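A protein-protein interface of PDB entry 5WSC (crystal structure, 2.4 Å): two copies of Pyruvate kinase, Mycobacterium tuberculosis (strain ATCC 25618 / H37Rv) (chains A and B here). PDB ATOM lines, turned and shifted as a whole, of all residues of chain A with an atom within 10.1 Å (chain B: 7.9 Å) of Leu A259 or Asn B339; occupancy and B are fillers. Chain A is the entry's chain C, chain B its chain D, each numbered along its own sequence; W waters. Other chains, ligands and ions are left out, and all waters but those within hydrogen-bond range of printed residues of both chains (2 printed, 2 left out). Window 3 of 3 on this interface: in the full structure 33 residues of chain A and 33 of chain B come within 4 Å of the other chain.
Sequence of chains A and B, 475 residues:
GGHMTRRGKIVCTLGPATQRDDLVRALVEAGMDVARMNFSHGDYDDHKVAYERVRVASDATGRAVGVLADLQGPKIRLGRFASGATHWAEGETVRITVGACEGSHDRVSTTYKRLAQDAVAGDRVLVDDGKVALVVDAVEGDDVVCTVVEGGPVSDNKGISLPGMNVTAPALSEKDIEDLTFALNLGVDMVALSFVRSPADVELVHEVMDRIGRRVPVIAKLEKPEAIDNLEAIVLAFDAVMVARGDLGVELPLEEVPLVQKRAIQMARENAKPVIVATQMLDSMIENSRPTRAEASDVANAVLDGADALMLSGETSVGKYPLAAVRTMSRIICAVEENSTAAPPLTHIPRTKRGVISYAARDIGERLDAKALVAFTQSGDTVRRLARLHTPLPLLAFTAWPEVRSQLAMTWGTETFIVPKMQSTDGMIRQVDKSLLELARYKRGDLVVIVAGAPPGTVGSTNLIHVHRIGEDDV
Water W2 lies within hydrogen-bond range of the side-chain carboxylate (OD1) of Asp A298 (2.4 Å), the side-chain hydroxyl (OG) of Ser B297 (2.9 Å) and the side-chain amide nitrogen (NE2) of Gln A261 (3.2 Å). Water W1 lies within hydrogen-bond range of the side-chain carboxylate (OD1) of Asp A305 (2.7 Å), the side-chain amino group (NZ) of Lys A262 (3.0 Å) and the side-chain amide oxygen (OD1) of Asn B301 (3.4 Å).
Of the 24 printed residues of chain A, 5 touch a printed residue of chain B. Hydrophobic or aromatic side chains of chain A within 4 Å of the printed part of chain B: Pro A258 and Leu A259. Of the 15 printed residues of chain B, 7 touch a printed residue of chain A. Along chain B the printed residues that touch a printed residue of chain A span positions 297 to 339. Among the printed residues, 7 pairs touch across the chains.
Ile B332 touches Glu A255 (CA to CB, 3.8 Å). Glu A255 touches Ala B335. Ala B300 touches Pro A258. Leu A259 touches Asn B339. Leu B304 touches Lys A262.
The side-chain amino group (NZ) of Lys A262 lies within hydrogen-bond range of the side-chain amide oxygen (OD1) of Asn B301 (2.9 Å). OG of Ser B297 is in hydrogen-bond range of OD1 of Asp A298 (2.9 Å).
NH1 of Arg A245 is in salt-bridge range of OD2 of Asp A298 (2.6 Å). NZ of Lys A262 lies within salt-bridge range of OD1 of Asp A305 (2.9 Å). The backbone carbonyl oxygen of Ser B297 lies within hydrogen-bond range of the side-chain amide nitrogen of Asn B301 (3.2 Å).
Leu A259 touches just one residue of chain B: Asn B339. Asn B339 touches one residue of chain A. No residue of chain A comes within 4 Å of Val B336. No residue of chain A comes within 4 Å of Ser B340. Printed residues of chain A within 4 Å of Ile B332: Glu A255. Printed residues of chain B within 4 Å of Lys A262: Asn B301 (2.9 Å) and Leu B304 (3.9 Å). Of the printed residues of chain A, Asn B301 touches Lys A262. Printed residues of chain A within 4 Å of Ala B300: Pro A258 (3.7 Å). Of the printed residues of chain A, Leu B304 touches Lys A262 (3.9 Å). Asp A305 touches none of the printed residues of chain B.
No position is printed for both chains. Of the 7 pairs that touch across the chains among the printed residues, none has its exchanged pair printed and touching as well.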
ATOM      1  N   LEU A 222      19.976  13.221  35.381  1.00  0.00           N
ATOM      2  CA  LEU A 222      20.685  12.099  34.784  1.00  0.00           C
ATOM      3  C   LEU A 222      21.605  12.535  33.658  1.00  0.00           C
ATOM      4  O   LEU A 222      21.170  12.710  32.551  1.00  0.00           O
ATOM      5  CB  LEU A 222      19.685  11.091  34.224  1.00  0.00           C
ATOM      6  CG  LEU A 222      18.643  10.626  35.245  1.00  0.00           C
ATOM      7  CD1 LEU A 222      17.636   9.680  34.630  1.00  0.00           C
ATOM      8  CD2 LEU A 222      19.297   9.983  36.445  1.00  0.00           C
ATOM      9  N   ILE A 228      23.288   6.286  35.265  1.00  0.00           N
ATOM     10  CA  ILE A 228      22.541   5.374  34.445  1.00  0.00           C
ATOM     11  C   ILE A 228      22.813   3.956  34.912  1.00  0.00           C
ATOM     12  O   ILE A 228      21.924   3.135  34.910  1.00  0.00           O
ATOM     13  CB  ILE A 228      22.880   5.543  32.956  1.00  0.00           C
ATOM     14  CG1 ILE A 228      22.674   6.977  32.520  1.00  0.00           C
ATOM     15  CG2 ILE A 228      21.968   4.696  32.104  1.00  0.00           C
ATOM     16  CD1 ILE A 228      21.254   7.456  32.792  1.00  0.00           C
ATOM     17  N   LEU A 231      20.429   3.372  37.826  1.00  0.00           N
ATOM     18  CA  LEU A 231      19.197   4.108  37.516  1.00  0.00           C
ATOM     19  C   LEU A 231      18.027   3.849  38.473  1.00  0.00           C
ATOM     20  O   LEU A 231      17.338   4.779  38.883  1.00  0.00           O
ATOM     21  CB  LEU A 231      18.730   3.786  36.098  1.00  0.00           C
ATOM     22  CG  LEU A 231      17.582   4.697  35.633  1.00  0.00           C
ATOM     23  CD1 LEU A 231      17.982   6.173  35.689  1.00  0.00           C
ATOM     24  CD2 LEU A 231      17.108   4.293  34.246  1.00  0.00           C
ATOM     25  N   VAL A 243      15.915  13.717  32.644  1.00  0.00           N
ATOM     26  CA  VAL A 243      16.820  13.328  31.626  1.00  0.00           C
ATOM     27  C   VAL A 243      17.516  14.608  31.099  1.00  0.00           C
ATOM     28  O   VAL A 243      16.897  15.414  30.398  1.00  0.00           O
ATOM     29  CB  VAL A 243      16.154  12.538  30.513  1.00  0.00           C
ATOM     30  CG1 VAL A 243      17.211  11.703  29.789  1.00  0.00           C
ATOM     31  CG2 VAL A 243      15.081  11.615  31.052  1.00  0.00           C
ATOM     32  N   ARG A 245      19.905  15.952  28.856  1.00  0.00           N
ATOM     33  CA  ARG A 245      20.518  15.345  27.688  1.00  0.00           C
ATOM     34  C   ARG A 245      21.741  16.105  27.179  1.00  0.00           C
ATOM     35  O   ARG A 245      22.591  15.533  26.513  1.00  0.00           O
ATOM     36  CB  ARG A 245      19.487  15.228  26.576  1.00  0.00           C
ATOM     37  CG  ARG A 245      18.198  14.560  27.036  1.00  0.00           C
ATOM     38  CD  ARG A 245      17.200  14.318  25.922  1.00  0.00           C
ATOM     39  NE  ARG A 245      16.944  15.514  25.146  1.00  0.00           N
ATOM     40  CZ  ARG A 245      16.163  15.524  24.070  1.00  0.00           C
ATOM     41  NH1 ARG A 245      16.006  16.643  23.384  1.00  0.00           N
ATOM     42  NH2 ARG A 245      15.525  14.405  23.675  1.00  0.00           N
ATOM     43  N   LEU A 248      24.459  14.677  29.276  1.00  0.00           N
ATOM     44  CA  LEU A 248      24.404  13.218  29.103  1.00  0.00           C
ATOM     45  C   LEU A 248      24.977  12.831  27.736  1.00  0.00           C
ATOM     46  O   LEU A 248      25.685  11.855  27.626  1.00  0.00           O
ATOM     47  CB  LEU A 248      22.972  12.695  29.254  1.00  0.00           C
ATOM     48  CG  LEU A 248      22.803  11.168  29.370  1.00  0.00           C
ATOM     49  CD1 LEU A 248      23.512  10.528  30.576  1.00  0.00           C
ATOM     50  CD2 LEU A 248      21.337  10.807  29.344  1.00  0.00           C
ATOM     51  N   LEU A 252      28.146  10.365  27.887  1.00  0.00           N
ATOM     52  CA  LEU A 252      27.975   9.084  27.167  1.00  0.00           C
ATOM     53  C   LEU A 252      28.002   9.322  25.666  1.00  0.00           C
ATOM     54  O   LEU A 252      27.723  10.431  25.215  1.00  0.00           O
ATOM     55  CB  LEU A 252      26.581   8.506  27.431  1.00  0.00           C
ATOM     56  CG  LEU A 252      26.258   7.929  28.804  1.00  0.00           C
ATOM     57  CD1 LEU A 252      24.883   7.313  28.775  1.00  0.00           C
ATOM     58  CD2 LEU A 252      27.319   6.878  29.176  1.00  0.00           C
ATOM     59  N   PRO A 253      28.230   8.253  24.874  1.00  0.00           N
ATOM     60  CA  PRO A 253      28.059   8.413  23.437  1.00  0.00           C
ATOM     61  C   PRO A 253      26.689   8.977  23.132  1.00  0.00           C
ATOM     62  O   PRO A 253      25.672   8.493  23.662  1.00  0.00           O
ATOM     63  CB  PRO A 253      28.165   7.007  22.905  1.00  0.00           C
ATOM     64  CG  PRO A 253      29.033   6.283  23.891  1.00  0.00           C
ATOM     65  CD  PRO A 253      28.805   6.954  25.229  1.00  0.00           C
ATOM     66  N   LEU A 254      26.652  10.007  22.298  1.00  0.00           N
ATOM     67  CA  LEU A 254      25.426  10.681  21.992  1.00  0.00           C
ATOM     68  C   LEU A 254      24.427   9.725  21.354  1.00  0.00           C
ATOM     69  O   LEU A 254      23.239   9.948  21.407  1.00  0.00           O
ATOM     70  CB  LEU A 254      25.715  11.911  21.104  1.00  0.00           C
ATOM     71  CG  LEU A 254      26.270  11.705  19.681  1.00  0.00           C
ATOM     72  CD1 LEU A 254      25.140  11.276  18.772  1.00  0.00           C
ATOM     73  CD2 LEU A 254      26.862  12.996  19.120  1.00  0.00           C
ATOM     74  N   GLU A 255      24.917   8.646  20.784  1.00  0.00           N
ATOM     75  CA  GLU A 255      24.053   7.695  20.106  1.00  0.00           C
ATOM     76  C   GLU A 255      23.275   6.802  21.083  1.00  0.00           C
ATOM     77  O   GLU A 255      22.268   6.194  20.695  1.00  0.00           O
ATOM     78  CB  GLU A 255      24.843   6.839  19.066  1.00  0.00           C
ATOM     79  CG  GLU A 255      25.950   5.979  19.633  1.00  0.00           C
ATOM     80  CD  GLU A 255      27.329   6.603  19.465  1.00  0.00           C
ATOM     81  OE1 GLU A 255      27.384   7.831  19.330  1.00  0.00           O
ATOM     82  OE2 GLU A 255      28.351   5.863  19.492  1.00  0.00           O
ATOM     83  N   GLU A 256      23.722   6.757  22.340  1.00  0.00           N
ATOM     84  CA  GLU A 256      23.080   5.923  23.352  1.00  0.00           C
ATOM     85  C   GLU A 256      21.974   6.691  24.100  1.00  0.00           C
ATOM     86  O   GLU A 256      21.188   6.103  24.868  1.00  0.00           O
ATOM     87  CB  GLU A 256      24.097   5.457  24.369  1.00  0.00           C
ATOM     88  CG  GLU A 256      25.180   4.515  23.916  1.00  0.00           C
ATOM     89  CD  GLU A 256      26.112   4.139  25.103  1.00  0.00           C
ATOM     90  OE1 GLU A 256      25.928   4.699  26.232  1.00  0.00           O
ATOM     91  OE2 GLU A 256      27.068   3.317  24.932  1.00  0.00           O
ATOM     92  N   VAL A 257      21.911   8.002  23.894  1.00  0.00           N
ATOM     93  CA  VAL A 257      21.035   8.804  24.691  1.00  0.00           C
ATOM     94  C   VAL A 257      19.547   8.488  24.453  1.00  0.00           C
ATOM     95  O   VAL A 257      18.754   8.499  25.390  1.00  0.00           O
ATOM     96  CB  VAL A 257      21.294  10.311  24.528  1.00  0.00           C
ATOM     97  CG1 VAL A 257      20.187  11.119  25.213  1.00  0.00           C
ATOM     98  CG2 VAL A 257      22.641  10.716  25.129  1.00  0.00           C
ATOM     99  N   PRO A 258      19.147   8.237  23.216  1.00  0.00           N
ATOM    100  CA  PRO A 258      17.710   8.073  23.014  1.00  0.00           C
ATOM    101  C   PRO A 258      17.103   6.885  23.718  1.00  0.00           C
ATOM    102  O   PRO A 258      15.962   6.955  24.167  1.00  0.00           O
ATOM    103  CB  PRO A 258      17.612   7.891  21.513  1.00  0.00           C
ATOM    104  CG  PRO A 258      18.716   8.764  20.998  1.00  0.00           C
ATOM    105  CD  PRO A 258      19.832   8.534  21.954  1.00  0.00           C
ATOM    106  N   LEU A 259      17.838   5.791  23.782  1.00  0.00           N
ATOM    107  CA  LEU A 259      17.376   4.636  24.534  1.00  0.00           C
ATOM    108  C   LEU A 259      17.550   4.829  26.028  1.00  0.00           C
ATOM    109  O   LEU A 259      16.800   4.229  26.834  1.00  0.00           O
ATOM    110  CB  LEU A 259      18.070   3.335  24.123  1.00  0.00           C
ATOM    111  CG  LEU A 259      17.808   2.812  22.723  1.00  0.00           C
ATOM    112  CD1 LEU A 259      18.169   1.341  22.623  1.00  0.00           C
ATOM    113  CD2 LEU A 259      16.385   3.026  22.261  1.00  0.00           C
ATOM    114  N   VAL A 260      18.530   5.621  26.441  1.00  0.00           N
ATOM    115  CA  VAL A 260      18.676   5.883  27.865  1.00  0.00           C
ATOM    116  C   VAL A 260      17.482   6.694  28.314  1.00  0.00           C
ATOM    117  O   VAL A 260      16.862   6.377  29.345  1.00  0.00           O
ATOM    118  CB  VAL A 260      19.996   6.574  28.210  1.00  0.00           C
ATOM    119  CG1 VAL A 260      19.941   7.179  29.613  1.00  0.00           C
ATOM    120  CG2 VAL A 260      21.143   5.562  28.140  1.00  0.00           C
ATOM    121  N   GLN A 261      17.128   7.707  27.515  1.00  0.00           N
ATOM    122  CA  GLN A 261      15.963   8.498  27.770  1.00  0.00           C
ATOM    123  C   GLN A 261      14.737   7.613  27.949  1.00  0.00           C
ATOM    124  O   GLN A 261      13.959   7.773  28.905  1.00  0.00           O
ATOM    125  CB  GLN A 261      15.711   9.498  26.617  1.00  0.00           C
ATOM    126  CG  GLN A 261      14.403  10.251  26.755  1.00  0.00           C
ATOM    127  CD  GLN A 261      14.166  11.236  25.641  1.00  0.00           C
ATOM    128  OE1 GLN A 261      15.075  11.984  25.259  1.00  0.00           O
ATOM    129  NE2 GLN A 261      12.927  11.221  25.075  1.00  0.00           N
ATOM    130  N   LYS A 262      14.531   6.695  27.030  1.00  0.00           N
ATOM    131  CA  LYS A 262      13.307   5.900  27.043  1.00  0.00           C
ATOM    132  C   LYS A 262      13.247   5.022  28.274  1.00  0.00           C
ATOM    133  O   LYS A 262      12.215   4.954  28.920  1.00  0.00           O
ATOM    134  CB  LYS A 262      13.174   5.118  25.762  1.00  0.00           C
ATOM    135  CG  LYS A 262      12.690   6.005  24.628  1.00  0.00           C
ATOM    136  CD  LYS A 262      13.143   5.459  23.272  1.00  0.00           C
ATOM    137  CE  LYS A 262      12.862   6.468  22.152  1.00  0.00           C
ATOM    138  NZ  LYS A 262      11.427   6.410  21.793  1.00  0.00           N
ATOM    139  N   ARG A 263      14.356   4.371  28.622  1.00  0.00           N
ATOM    140  CA  ARG A 263      14.445   3.561  29.857  1.00  0.00           C
ATOM    141  C   ARG A 263      14.226   4.375  31.120  1.00  0.00           C
ATOM    142  O   ARG A 263      13.656   3.888  32.073  1.00  0.00           O
ATOM    143  CB  ARG A 263      15.828   2.874  29.941  1.00  0.00           C
ATOM    144  CG  ARG A 263      16.318   2.378  31.320  1.00  0.00           C
ATOM    145  CD  ARG A 263      17.611   1.583  31.138  1.00  0.00           C
ATOM    146  NE  ARG A 263      18.141   0.978  32.363  1.00  0.00           N
ATOM    147  CZ  ARG A 263      19.429   1.009  32.738  1.00  0.00           C
ATOM    148  NH1 ARG A 263      20.319   1.629  31.997  1.00  0.00           N
ATOM    149  NH2 ARG A 263      19.839   0.436  33.886  1.00  0.00           N
ATOM    150  N   ALA A 264      14.683   5.606  31.145  1.00  0.00           N
ATOM    151  CA  ALA A 264      14.660   6.339  32.385  1.00  0.00           C
ATOM    152  C   ALA A 264      13.235   6.847  32.635  1.00  0.00           C
ATOM    153  O   ALA A 264      12.787   6.903  33.758  1.00  0.00           O
ATOM    154  CB  ALA A 264      15.644   7.475  32.329  1.00  0.00           C
ATOM    155  N   ILE A 265      12.545   7.210  31.566  1.00  0.00           N
ATOM    156  CA  ILE A 265      11.131   7.541  31.625  1.00  0.00           C
ATOM    157  C   ILE A 265      10.285   6.378  32.114  1.00  0.00           C
ATOM    158  O   ILE A 265       9.378   6.552  32.939  1.00  0.00           O
ATOM    159  CB  ILE A 265      10.619   8.016  30.226  1.00  0.00           C
ATOM    160  CG1 ILE A 265      11.143   9.429  29.943  1.00  0.00           C
ATOM    161  CG2 ILE A 265       9.107   8.063  30.197  1.00  0.00           C
ATOM    162  CD1 ILE A 265      10.958   9.892  28.519  1.00  0.00           C
ATOM    163  N   GLN A 266      10.558   5.185  31.591  1.00  0.00           N
ATOM    164  CA  GLN A 266       9.807   4.000  31.972  1.00  0.00           C
ATOM    165  C   GLN A 266      10.061   3.729  33.456  1.00  0.00           C
ATOM    166  O   GLN A 266       9.164   3.340  34.164  1.00  0.00           O
ATOM    167  CB  GLN A 266      10.249   2.780  31.139  1.00  0.00           C
ATOM    168  CG  GLN A 266       9.476   1.483  31.398  1.00  0.00           C
ATOM    169  CD  GLN A 266       8.052   1.486  30.852  1.00  0.00           C
ATOM    170  OE1 GLN A 266       7.708   2.248  29.935  1.00  0.00           O
ATOM    171  NE2 GLN A 266       7.205   0.610  31.419  1.00  0.00           N
ATOM    172  N   MET A 267      11.292   3.916  33.902  1.00  0.00           N
ATOM    173  CA  MET A 267      11.691   3.590  35.267  1.00  0.00           C
ATOM    174  C   MET A 267      10.992   4.594  36.254  1.00  0.00           C
ATOM    175  O   MET A 267      10.447   4.222  37.321  1.00  0.00           O
ATOM    176  CB  MET A 267      13.229   3.689  35.318  1.00  0.00           C
ATOM    177  CG  MET A 267      13.867   3.575  36.658  1.00  0.00           C
ATOM    178  SD  MET A 267      14.035   1.876  37.020  1.00  0.00           S
ATOM    179  CE  MET A 267      15.205   1.387  35.738  1.00  0.00           C
ATOM    180  N   ASP A 298      11.169  15.272  18.113  1.00  0.00           N
ATOM    181  CA  ASP A 298      11.795  14.926  19.384  1.00  0.00           C
ATOM    182  C   ASP A 298      10.796  15.122  20.509  1.00  0.00           C
ATOM    183  O   ASP A 298      10.628  14.248  21.393  1.00  0.00           O
ATOM    184  CB  ASP A 298      13.042  15.798  19.608  1.00  0.00           C
ATOM    185  CG  ASP A 298      13.712  15.528  20.897  1.00  0.00           C
ATOM    186  OD1 ASP A 298      13.858  14.381  21.228  1.00  0.00           O
ATOM    187  OD2 ASP A 298      14.128  16.480  21.591  1.00  0.00           O
ATOM    188  N   ASP A 305       6.800   8.584  24.662  1.00  0.00           N
ATOM    189  CA  ASP A 305       7.613   7.860  25.637  1.00  0.00           C
ATOM    190  C   ASP A 305       6.910   7.790  26.974  1.00  0.00           C
ATOM    191  O   ASP A 305       7.151   6.892  27.764  1.00  0.00           O
ATOM    192  CB  ASP A 305       8.969   8.540  25.832  1.00  0.00           C
ATOM    193  CG  ASP A 305       9.884   8.348  24.646  1.00  0.00           C
ATOM    194  OD1 ASP A 305       9.662   7.383  23.872  1.00  0.00           O
ATOM    195  OD2 ASP A 305      10.826   9.154  24.478  1.00  0.00           O
ATOM    196  N   SER B 297      17.731  11.866  18.610  1.00  0.00           N
ATOM    197  CA  SER B 297      16.434  11.296  18.881  1.00  0.00           C
ATOM    198  C   SER B 297      15.637  11.049  17.607  1.00  0.00           C
ATOM    199  O   SER B 297      14.973   9.984  17.464  1.00  0.00           O
ATOM    200  CB  SER B 297      15.652  12.264  19.788  1.00  0.00           C
ATOM    201  OG  SER B 297      14.332  11.802  20.043  1.00  0.00           O
ATOM    202  N   ALA B 300      16.833   8.080  15.816  1.00  0.00           N
ATOM    203  CA  ALA B 300      16.516   6.839  16.544  1.00  0.00           C
ATOM    204  C   ALA B 300      15.030   6.467  16.434  1.00  0.00           C
ATOM    205  O   ALA B 300      14.679   5.307  16.372  1.00  0.00           O
ATOM    206  CB  ALA B 300      16.932   6.923  17.992  1.00  0.00           C
ATOM    207  N   ASN B 301      14.160   7.449  16.407  1.00  0.00           N
ATOM    208  CA  ASN B 301      12.735   7.183  16.460  1.00  0.00           C
ATOM    209  C   ASN B 301      12.204   6.855  15.086  1.00  0.00           C
ATOM    210  O   ASN B 301      11.128   6.311  14.962  1.00  0.00           O
ATOM    211  CB  ASN B 301      11.981   8.401  17.099  1.00  0.00           C
ATOM    212  CG  ASN B 301      11.875   8.288  18.604  1.00  0.00           C
ATOM    213  OD1 ASN B 301      11.210   7.383  19.097  1.00  0.00           O
ATOM    214  ND2 ASN B 301      12.512   9.218  19.354  1.00  0.00           N
ATOM    215  N   LEU B 304      12.863   3.152  15.114  1.00  0.00           N
ATOM    216  CA  LEU B 304      11.863   2.413  15.869  1.00  0.00           C
ATOM    217  C   LEU B 304      10.509   2.458  15.197  1.00  0.00           C
ATOM    218  O   LEU B 304       9.707   1.511  15.330  1.00  0.00           O
ATOM    219  CB  LEU B 304      11.736   2.966  17.278  1.00  0.00           C
ATOM    220  CG  LEU B 304      13.061   2.974  18.043  1.00  0.00           C
ATOM    221  CD1 LEU B 304      13.046   3.958  19.194  1.00  0.00           C
ATOM    222  CD2 LEU B 304      13.428   1.577  18.545  1.00  0.00           C
ATOM    223  N   ILE B 332      24.008   6.117  15.207  1.00  0.00           N
ATOM    224  CA  ILE B 332      22.720   6.158  15.934  1.00  0.00           C
ATOM    225  C   ILE B 332      21.801   4.994  15.511  1.00  0.00           C
ATOM    226  O   ILE B 332      21.122   4.362  16.352  1.00  0.00           O
ATOM    227  CB  ILE B 332      21.969   7.459  15.653  1.00  0.00           C
ATOM    228  CG1 ILE B 332      22.698   8.633  16.274  1.00  0.00           C
ATOM    229  CG2 ILE B 332      20.572   7.425  16.221  1.00  0.00           C
ATOM    230  CD1 ILE B 332      22.431   9.973  15.598  1.00  0.00           C
ATOM    231  N   ILE B 333      21.759   4.703  14.217  1.00  0.00           N
ATOM    232  CA  ILE B 333      20.958   3.591  13.761  1.00  0.00           C
ATOM    233  C   ILE B 333      21.456   2.304  14.381  1.00  0.00           C
ATOM    234  O   ILE B 333      20.666   1.480  14.817  1.00  0.00           O
ATOM    235  CB  ILE B 333      20.980   3.458  12.232  1.00  0.00           C
ATOM    236  CG1 ILE B 333      20.256   4.646  11.590  1.00  0.00           C
ATOM    237  CG2 ILE B 333      20.319   2.145  11.798  1.00  0.00           C
ATOM    238  CD1 ILE B 333      20.502   4.754  10.094  1.00  0.00           C
ATOM    239  N   CYS B 334      22.764   2.107  14.380  1.00  0.00           N
ATOM    240  CA  CYS B 334      23.342   0.876  14.880  1.00  0.00           C
ATOM    241  C   CYS B 334      23.109   0.752  16.368  1.00  0.00           C
ATOM    242  O   CYS B 334      22.921  -0.372  16.876  1.00  0.00           O
ATOM    243  CB  CYS B 334      24.844   0.811  14.568  1.00  0.00           C
ATOM    244  SG  CYS B 334      25.197   0.447  12.810  1.00  0.00           S
ATOM    245  N   ALA B 335      23.122   1.885  17.070  1.00  0.00           N
ATOM    246  CA  ALA B 335      22.943   1.883  18.511  1.00  0.00           C
ATOM    247  C   ALA B 335      21.540   1.381  18.834  1.00  0.00           C
ATOM    248  O   ALA B 335      21.351   0.564  19.699  1.00  0.00           O
ATOM    249  CB  ALA B 335      23.149   3.279  19.073  1.00  0.00           C
ATOM    250  N   VAL B 336      20.561   1.840  18.090  1.00  0.00           N
ATOM    251  CA  VAL B 336      19.190   1.399  18.306  1.00  0.00           C
ATOM    252  C   VAL B 336      19.024  -0.069  17.952  1.00  0.00           C
ATOM    253  O   VAL B 336      18.351  -0.821  18.672  1.00  0.00           O
ATOM    254  CB  VAL B 336      18.208   2.245  17.491  1.00  0.00           C
ATOM    255  CG1 VAL B 336      16.804   1.652  17.515  1.00  0.00           C
ATOM    256  CG2 VAL B 336      18.195   3.663  18.037  1.00  0.00           C
ATOM    257  N   GLU B 337      19.655  -0.485  16.854  1.00  0.00           N
ATOM    258  CA  GLU B 337      19.553  -1.852  16.345  1.00  0.00           C
ATOM    259  C   GLU B 337      20.248  -2.891  17.217  1.00  0.00           C
ATOM    260  O   GLU B 337      19.790  -4.033  17.340  1.00  0.00           O
ATOM    261  CB  GLU B 337      20.056  -1.915  14.898  1.00  0.00           C
ATOM    262  CG  GLU B 337      19.031  -1.370  13.899  1.00  0.00           C
ATOM    263  CD  GLU B 337      19.594  -1.154  12.511  1.00  0.00           C
ATOM    264  OE1 GLU B 337      20.774  -1.552  12.271  1.00  0.00           O
ATOM    265  OE2 GLU B 337      18.841  -0.603  11.660  1.00  0.00           O
ATOM    266  N   GLU B 338      21.362  -2.501  17.814  1.00  0.00           N
ATOM    267  CA  GLU B 338      22.051  -3.386  18.743  1.00  0.00           C
ATOM    268  C   GLU B 338      21.146  -3.692  19.906  1.00  0.00           C
ATOM    269  O   GLU B 338      21.119  -4.808  20.392  1.00  0.00           O
ATOM    270  CB  GLU B 338      23.395  -2.777  19.134  1.00  0.00           C
ATOM    271  CG  GLU B 338      24.236  -2.614  17.845  1.00  0.00           C
ATOM    272  CD  GLU B 338      25.743  -2.503  18.014  1.00  0.00           C
ATOM    273  OE1 GLU B 338      26.345  -3.302  18.812  1.00  0.00           O
ATOM    274  OE2 GLU B 338      26.342  -1.641  17.291  1.00  0.00           O
ATOM    275  N   ASN B 339      20.340  -2.717  20.317  1.00  0.00           N
ATOM    276  CA  ASN B 339      19.286  -2.993  21.295  1.00  0.00           C
ATOM    277  C   ASN B 339      18.187  -3.945  20.747  1.00  0.00           C
ATOM    278  O   ASN B 339      17.990  -5.048  21.272  1.00  0.00           O
ATOM    279  CB  ASN B 339      18.617  -1.726  21.759  1.00  0.00           C
ATOM    280  CG  ASN B 339      17.545  -2.009  22.777  1.00  0.00           C
ATOM    281  OD1 ASN B 339      16.355  -2.120  22.446  1.00  0.00           O
ATOM    282  ND2 ASN B 339      17.973  -2.214  24.028  1.00  0.00           N
ATOM    283  N   SER B 340      17.462  -3.501  19.729  1.00  0.00           N
ATOM    284  CA  SER B 340      16.412  -4.324  19.111  1.00  0.00           C
ATOM    285  C   SER B 340      16.169  -3.894  17.684  1.00  0.00           C
ATOM    286  O   SER B 340      16.229  -2.701  17.400  1.00  0.00           O
ATOM    287  CB  SER B 340      15.097  -4.172  19.868  1.00  0.00           C
ATOM    288  OG  SER B 340      14.139  -5.053  19.318  1.00  0.00           O
ATOM    289  N   THR B 341      15.894  -4.864  16.800  1.00  0.00           N
ATOM    290  CA  THR B 341      15.413  -4.566  15.452  1.00  0.00           C
ATOM    291  C   THR B 341      13.880  -4.582  15.343  1.00  0.00           C
ATOM    292  O   THR B 341      13.312  -4.345  14.263  1.00  0.00           O
ATOM    293  CB  THR B 341      16.018  -5.514  14.376  1.00  0.00           C
ATOM    294  OG1 THR B 341      15.673  -6.872  14.642  1.00  0.00           O
ATOM    295  CG2 THR B 341      17.566  -5.375  14.305  1.00  0.00           C
ATOM    296  N   ALA B 342      13.187  -4.834  16.442  1.00  0.00           N
ATOM    297  CA  ALA B 342      11.730  -5.004  16.375  1.00  0.00           C
ATOM    298  C   ALA B 342      11.074  -3.754  15.794  1.00  0.00           C
ATOM    299  O   ALA B 342      11.523  -2.661  16.040  1.00  0.00           O
ATOM    300  CB  ALA B 342      11.144  -5.333  17.764  1.00  0.00           C
HETATM  301  O   HOH W   1       8.768   7.760  21.406  1.00  0.00           O
HETATM  302  O   HOH W   2      12.539  12.538  22.135  1.00  0.00           O
